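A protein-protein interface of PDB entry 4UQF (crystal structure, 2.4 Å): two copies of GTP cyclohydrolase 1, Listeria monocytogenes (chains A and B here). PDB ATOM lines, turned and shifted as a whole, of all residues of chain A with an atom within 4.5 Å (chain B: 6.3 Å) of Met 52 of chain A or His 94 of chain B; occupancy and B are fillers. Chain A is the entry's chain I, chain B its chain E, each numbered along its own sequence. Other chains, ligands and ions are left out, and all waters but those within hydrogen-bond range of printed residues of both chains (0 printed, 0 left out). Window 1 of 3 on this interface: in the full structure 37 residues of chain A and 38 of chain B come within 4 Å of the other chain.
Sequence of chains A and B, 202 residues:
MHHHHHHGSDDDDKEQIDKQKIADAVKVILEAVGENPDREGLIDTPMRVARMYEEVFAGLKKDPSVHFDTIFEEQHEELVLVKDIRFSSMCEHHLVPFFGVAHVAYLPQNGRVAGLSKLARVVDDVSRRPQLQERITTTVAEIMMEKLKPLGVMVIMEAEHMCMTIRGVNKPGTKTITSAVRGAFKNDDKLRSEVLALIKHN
No position is printed for both chains.
Of the printed residues of chain B, Arg 48 of chain A touches His 93 (3.0 Å) and His 94 (3.9 Å).
Of the printed residues of chain B, Val 49 of chain A touches His 94 (3.4 Å).
Printed residues of chain B within 4 Å of Met 52 of chain A: His 94 (3.99 Å) and Arg 167 (3.4 Å).
Of the printed residues of chain A, His 94 of chain B touches Arg 48 (3.9 Å), Val 49 (3.4 Å) and Met 52 (3.99 Å).
The nearest printed residue of chain B that does not touch Met 52 of chain A is Ile 166 of chain B (4.1 Å).
The nearest printed residue of chain A that does not touch His 93 of chain B is Val 49 of chain A (4.2 Å).
The backbone carbonyl oxygen (O) of His 93 of chain B is in hydrogen-bond range of the guanidinium group (NE) of Arg 48 of chain A (3.0 Å).
The backbone NH (N) of His 94 of chain B sits at hydrogen-bond distance from the side-chain sulfur (SG) of Cys 91 of chain B (3.4 Å).
The side-chain sulfur (SG) of Cys 163 of chain B lies within hydrogen-bond range of a ring nitrogen (ND1) of His 94 of chain B, at 2.4 Å.
O of Cys 163 of chain B sits at hydrogen-bond distance from NH1 of Arg 167 of chain B (2.9 Å).
The side-chain sulfur (SG) of Cys 91 of chain B forms a disulfide with the side-chain sulfur (SG) of Cys 163 of chain B (2.1 Å).
Among the printed residues, pairs that only touch across the chains: Arg 48 of chain A with His 94 of chain B, Val 49 of chain A with His 94 of chain B, Met 52 of chain A with His 94 of chain B, Met 52 of chain A with Arg 167 of chain B, Glu 55 of chain A with Arg 167 of chain B and Val 56 of chain A with Ile 166 of chain B.
Of the 10 printed residues of chain B, 4 touch a printed residue of chain A.
Printed residues of chain B that touch a printed residue of chain A: His 93, His 94, Ile 166 and Arg 167.
Along chain B the printed residues that touch a printed residue of chain A span positions 93 to 167.
Of the 9 printed residues of chain A, 5 touch a printed residue of chain B.
Printed residues of chain A that touch a printed residue of chain B: Arg 48, Val 49, Met 52, Glu 55 and Val 56.
Among the printed residues, 7 pairs touch across the chains.
Among the printed residues, no Asp or Glu carboxylate lies within 4 Å of a Lys or Arg side-chain nitrogen of the other chain.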
ATOM      1  N   ARG A  48      35.022  22.197 -29.553  1.00  0.00           N
ATOM      2  CA  ARG A  48      34.061  21.160 -29.213  1.00  0.00           C
ATOM      3  C   ARG A  48      32.880  21.210 -30.155  1.00  0.00           C
ATOM      4  O   ARG A  48      32.413  20.181 -30.643  1.00  0.00           O
ATOM      5  CB  ARG A  48      33.580  21.307 -27.781  1.00  0.00           C
ATOM      6  CG  ARG A  48      34.500  20.673 -26.760  1.00  0.00           C
ATOM      7  CD  ARG A  48      33.855  20.653 -25.394  1.00  0.00           C
ATOM      8  NE  ARG A  48      33.676  22.017 -24.896  1.00  0.00           N
ATOM      9  CZ  ARG A  48      34.278  22.529 -23.827  1.00  0.00           C
ATOM     10  NH1 ARG A  48      35.115  21.788 -23.108  1.00  0.00           N
ATOM     11  NH2 ARG A  48      34.037  23.790 -23.468  1.00  0.00           N
ATOM     12  N   VAL A  49      32.406  22.420 -30.442  1.00  0.00           N
ATOM     13  CA  VAL A  49      31.309  22.576 -31.403  1.00  0.00           C
ATOM     14  C   VAL A  49      31.748  22.117 -32.787  1.00  0.00           C
ATOM     15  O   VAL A  49      31.001  21.421 -33.476  1.00  0.00           O
ATOM     16  CB  VAL A  49      30.776  24.021 -31.431  1.00  0.00           C
ATOM     17  CG1 VAL A  49      29.760  24.193 -32.520  1.00  0.00           C
ATOM     18  CG2 VAL A  49      30.123  24.336 -30.101  1.00  0.00           C
ATOM     19  N   ALA A  50      32.973  22.446 -33.175  1.00  0.00           N
ATOM     20  CA  ALA A  50      33.484  21.976 -34.463  1.00  0.00           C
ATOM     21  C   ALA A  50      33.507  20.445 -34.551  1.00  0.00           C
ATOM     22  O   ALA A  50      33.020  19.880 -35.523  1.00  0.00           O
ATOM     23  CB  ALA A  50      34.860  22.541 -34.738  1.00  0.00           C
ATOM     24  N   ARG A  51      34.026  19.783 -33.511  1.00  0.00           N
ATOM     25  CA  ARG A  51      34.091  18.307 -33.484  1.00  0.00           C
ATOM     26  C   ARG A  51      32.715  17.684 -33.459  1.00  0.00           C
ATOM     27  O   ARG A  51      32.447  16.682 -34.118  1.00  0.00           O
ATOM     28  CB  ARG A  51      34.895  17.815 -32.290  1.00  0.00           C
ATOM     29  CG  ARG A  51      36.386  18.019 -32.451  1.00  0.00           C
ATOM     30  CD  ARG A  51      37.167  17.266 -31.398  1.00  0.00           C
ATOM     31  NE  ARG A  51      36.991  17.876 -30.078  1.00  0.00           N
ATOM     32  CZ  ARG A  51      37.781  18.812 -29.545  1.00  0.00           C
ATOM     33  NH1 ARG A  51      38.834  19.284 -30.206  1.00  0.00           N
ATOM     34  NH2 ARG A  51      37.517  19.279 -28.329  1.00  0.00           N
ATOM     35  N   MET A  52      31.798  18.328 -32.756  1.00  0.00           N
ATOM     36  CA  MET A  52      30.430  17.865 -32.784  1.00  0.00           C
ATOM     37  C   MET A  52      29.815  17.960 -34.182  1.00  0.00           C
ATOM     38  O   MET A  52      29.195  17.015 -34.656  1.00  0.00           O
ATOM     39  CB  MET A  52      29.601  18.676 -31.819  1.00  0.00           C
ATOM     40  CG  MET A  52      28.191  18.135 -31.739  1.00  0.00           C
ATOM     41  SD  MET A  52      27.120  19.221 -30.873  1.00  0.00           S
ATOM     42  CE  MET A  52      26.914  20.552 -32.090  1.00  0.00           C
ATOM     43  N   TYR A  53      29.980  19.098 -34.858  1.00  0.00           N
ATOM     44  CA  TYR A  53      29.429  19.236 -36.201  1.00  0.00           C
ATOM     45  C   TYR A  53      30.035  18.209 -37.143  1.00  0.00           C
ATOM     46  O   TYR A  53      29.348  17.663 -38.007  1.00  0.00           O
ATOM     47  CB  TYR A  53      29.630  20.644 -36.730  1.00  0.00           C
ATOM     48  CG  TYR A  53      28.666  21.669 -36.181  1.00  0.00           C
ATOM     49  CD1 TYR A  53      27.415  21.313 -35.703  1.00  0.00           C
ATOM     50  CD2 TYR A  53      28.999  23.009 -36.182  1.00  0.00           C
ATOM     51  CE1 TYR A  53      26.525  22.265 -35.233  1.00  0.00           C
ATOM     52  CE2 TYR A  53      28.124  23.970 -35.710  1.00  0.00           C
ATOM     53  CZ  TYR A  53      26.891  23.594 -35.252  1.00  0.00           C
ATOM     54  OH  TYR A  53      26.038  24.551 -34.791  1.00  0.00           O
ATOM     55  N   GLU A  54      31.315  17.924 -36.965  1.00  0.00           N
ATOM     56  CA  GLU A  54      31.951  16.921 -37.785  1.00  0.00           C
ATOM     57  C   GLU A  54      31.251  15.585 -37.645  1.00  0.00           C
ATOM     58  O   GLU A  54      31.057  14.888 -38.636  1.00  0.00           O
ATOM     59  CB  GLU A  54      33.419  16.803 -37.409  1.00  0.00           C
ATOM     60  CG  GLU A  54      34.204  15.791 -38.212  1.00  0.00           C
ATOM     61  CD  GLU A  54      35.692  15.921 -37.966  1.00  0.00           C
ATOM     62  OE1 GLU A  54      36.130  15.735 -36.826  1.00  0.00           O
ATOM     63  OE2 GLU A  54      36.433  16.241 -38.897  1.00  0.00           O
ATOM     64  N   GLU A  55      30.840  15.254 -36.426  1.00  0.00           N
ATOM     65  CA  GLU A  55      30.193  13.966 -36.172  1.00  0.00           C
ATOM     66  C   GLU A  55      28.752  13.968 -36.617  1.00  0.00           C
ATOM     67  O   GLU A  55      28.356  13.115 -37.415  1.00  0.00           O
ATOM     68  CB  GLU A  55      30.359  13.505 -34.719  1.00  0.00           C
ATOM     69  CG  GLU A  55      30.511  12.003 -34.498  1.00  0.00           C
ATOM     70  CD  GLU A  55      31.042  11.680 -33.100  1.00  0.00           C
ATOM     71  OE1 GLU A  55      30.806  12.483 -32.146  1.00  0.00           O
ATOM     72  OE2 GLU A  55      31.656  10.587 -32.925  1.00  0.00           O
ATOM     73  N   VAL A  56      27.976  14.962 -36.193  1.00  0.00           N
ATOM     74  CA  VAL A  56      26.529  14.973 -36.523  1.00  0.00           C
ATOM     75  C   VAL A  56      26.195  15.328 -37.974  1.00  0.00           C
ATOM     76  O   VAL A  56      25.099  15.042 -38.435  1.00  0.00           O
ATOM     77  CB  VAL A  56      25.687  15.881 -35.595  1.00  0.00           C
ATOM     78  CG1 VAL A  56      25.974  15.557 -34.143  1.00  0.00           C
ATOM     79  CG2 VAL A  56      25.903  17.353 -35.861  1.00  0.00           C
ATOM     80  N   CYS B  91      24.048  23.662 -23.318  1.00  0.00           N
ATOM     81  CA  CYS B  91      25.317  23.335 -22.651  1.00  0.00           C
ATOM     82  C   CYS B  91      26.283  24.377 -23.161  1.00  0.00           C
ATOM     83  O   CYS B  91      26.284  24.725 -24.334  1.00  0.00           O
ATOM     84  CB  CYS B  91      25.839  21.851 -22.801  1.00  0.00           C
ATOM     85  SG  CYS B  91      26.268  21.163 -24.433  1.00  0.00           S
ATOM     86  N   GLU B  92      27.111  24.889 -22.278  1.00  0.00           N
ATOM     87  CA  GLU B  92      28.149  25.794 -22.703  1.00  0.00           C
ATOM     88  C   GLU B  92      29.261  25.078 -23.482  1.00  0.00           C
ATOM     89  O   GLU B  92      30.034  25.715 -24.204  1.00  0.00           O
ATOM     90  CB  GLU B  92      28.700  26.584 -21.499  1.00  0.00           C
ATOM     91  CG  GLU B  92      29.428  25.768 -20.425  1.00  0.00           C
ATOM     92  CD  GLU B  92      29.825  26.625 -19.241  1.00  0.00           C
ATOM     93  OE1 GLU B  92      29.175  27.674 -19.009  1.00  0.00           O
ATOM     94  OE2 GLU B  92      30.823  26.276 -18.570  1.00  0.00           O
ATOM     95  N   HIS B  93      29.399  23.770 -23.301  1.00  0.00           N
ATOM     96  CA  HIS B  93      30.461  23.048 -23.989  1.00  0.00           C
ATOM     97  C   HIS B  93      30.210  22.883 -25.477  1.00  0.00           C
ATOM     98  O   HIS B  93      31.161  22.917 -26.249  1.00  0.00           O
ATOM     99  CB  HIS B  93      30.701  21.699 -23.338  1.00  0.00           C
ATOM    100  CG  HIS B  93      30.923  21.806 -21.891  1.00  0.00           C
ATOM    101  ND1 HIS B  93      31.705  22.797 -21.334  1.00  0.00           N
ATOM    102  CD2 HIS B  93      30.436  21.075 -20.870  1.00  0.00           C
ATOM    103  CE1 HIS B  93      31.712  22.645 -20.021  1.00  0.00           C
ATOM    104  NE2 HIS B  93      30.948  21.611 -19.718  1.00  0.00           N
ATOM    105  N   HIS B  94      28.949  22.672 -25.855  1.00  0.00           N
ATOM    106  CA  HIS B  94      28.582  22.334 -27.230  1.00  0.00           C
ATOM    107  C   HIS B  94      27.485  23.185 -27.810  1.00  0.00           C
ATOM    108  O   HIS B  94      27.166  23.036 -28.972  1.00  0.00           O
ATOM    109  CB  HIS B  94      28.119  20.892 -27.317  1.00  0.00           C
ATOM    110  CG  HIS B  94      29.138  19.917 -26.852  1.00  0.00           C
ATOM    111  ND1 HIS B  94      29.216  19.499 -25.540  1.00  0.00           N
ATOM    112  CD2 HIS B  94      30.140  19.293 -27.510  1.00  0.00           C
ATOM    113  CE1 HIS B  94      30.235  18.672 -25.411  1.00  0.00           C
ATOM    114  NE2 HIS B  94      30.810  18.528 -26.590  1.00  0.00           N
ATOM    115  N   LEU B  95      26.908  24.054 -27.001  1.00  0.00           N
ATOM    116  CA  LEU B  95      25.790  24.893 -27.414  1.00  0.00           C
ATOM    117  C   LEU B  95      24.641  24.089 -27.968  1.00  0.00           C
ATOM    118  O   LEU B  95      24.025  24.455 -28.958  1.00  0.00           O
ATOM    119  CB  LEU B  95      26.245  25.946 -28.417  1.00  0.00           C
ATOM    120  CG  LEU B  95      27.378  26.844 -27.938  1.00  0.00           C
ATOM    121  CD1 LEU B  95      27.746  27.799 -29.045  1.00  0.00           C
ATOM    122  CD2 LEU B  95      27.000  27.618 -26.681  1.00  0.00           C
ATOM    123  N   VAL B  96      24.350  22.979 -27.319  1.00  0.00           N
ATOM    124  CA  VAL B  96      23.196  22.214 -27.682  1.00  0.00           C
ATOM    125  C   VAL B  96      22.292  22.082 -26.453  1.00  0.00           C
ATOM    126  O   VAL B  96      22.766  22.065 -25.304  1.00  0.00           O
ATOM    127  CB  VAL B  96      23.570  20.922 -28.432  1.00  0.00           C
ATOM    128  CG1 VAL B  96      23.842  19.736 -27.528  1.00  0.00           C
ATOM    129  CG2 VAL B  96      22.466  20.560 -29.404  1.00  0.00           C
ATOM    130  N   MET B 162      21.499  16.642 -24.924  1.00  0.00           N
ATOM    131  CA  MET B 162      21.751  16.300 -26.312  1.00  0.00           C
ATOM    132  C   MET B 162      23.265  16.285 -26.622  1.00  0.00           C
ATOM    133  O   MET B 162      23.660  15.479 -27.440  1.00  0.00           O
ATOM    134  CB  MET B 162      21.021  17.268 -27.246  1.00  0.00           C
ATOM    135  CG  MET B 162      19.552  17.515 -26.943  1.00  0.00           C
ATOM    136  SD  MET B 162      18.462  16.214 -27.576  1.00  0.00           S
ATOM    137  CE  MET B 162      18.391  15.079 -26.186  1.00  0.00           C
ATOM    138  N   CYS B 163      24.077  17.144 -25.947  1.00  0.00           N
ATOM    139  CA  CYS B 163      25.587  17.061 -25.850  1.00  0.00           C
ATOM    140  C   CYS B 163      25.888  15.499 -26.039  1.00  0.00           C
ATOM    141  O   CYS B 163      26.782  15.087 -26.784  1.00  0.00           O
ATOM    142  CB  CYS B 163      26.172  17.739 -24.461  1.00  0.00           C
ATOM    143  SG  CYS B 163      27.256  19.307 -24.148  1.00  0.00           S
ATOM    144  N   ILE B 166      23.123  12.868 -29.370  1.00  0.00           N
ATOM    145  CA  ILE B 166      23.283  13.043 -30.813  1.00  0.00           C
ATOM    146  C   ILE B 166      24.705  12.829 -31.268  1.00  0.00           C
ATOM    147  O   ILE B 166      24.979  12.837 -32.458  1.00  0.00           O
ATOM    148  CB  ILE B 166      22.875  14.484 -31.255  1.00  0.00           C
ATOM    149  CG1 ILE B 166      23.899  15.515 -30.739  1.00  0.00           C
ATOM    150  CG2 ILE B 166      21.469  14.797 -30.764  1.00  0.00           C
ATOM    151  CD1 ILE B 166      23.708  16.933 -31.211  1.00  0.00           C
ATOM    152  N   ARG B 167      25.628  12.751 -30.328  1.00  0.00           N
ATOM    153  CA  ARG B 167      27.040  12.753 -30.686  1.00  0.00           C
ATOM    154  C   ARG B 167      27.572  11.344 -30.730  1.00  0.00           C
ATOM    155  O   ARG B 167      26.829  10.399 -30.534  1.00  0.00           O
ATOM    156  CB  ARG B 167      27.825  13.665 -29.735  1.00  0.00           C
ATOM    157  CG  ARG B 167      28.405  14.880 -30.426  1.00  0.00           C
ATOM    158  CD  ARG B 167      29.106  15.795 -29.467  1.00  0.00           C
ATOM    159  NE  ARG B 167      30.333  15.211 -28.904  1.00  0.00           N
ATOM    160  CZ  ARG B 167      30.556  14.948 -27.609  1.00  0.00           C
ATOM    161  NH1 ARG B 167      29.663  15.214 -26.657  1.00  0.00           N
ATOM    162  NH2 ARG B 167      31.718  14.403 -27.251  1.00  0.00           N
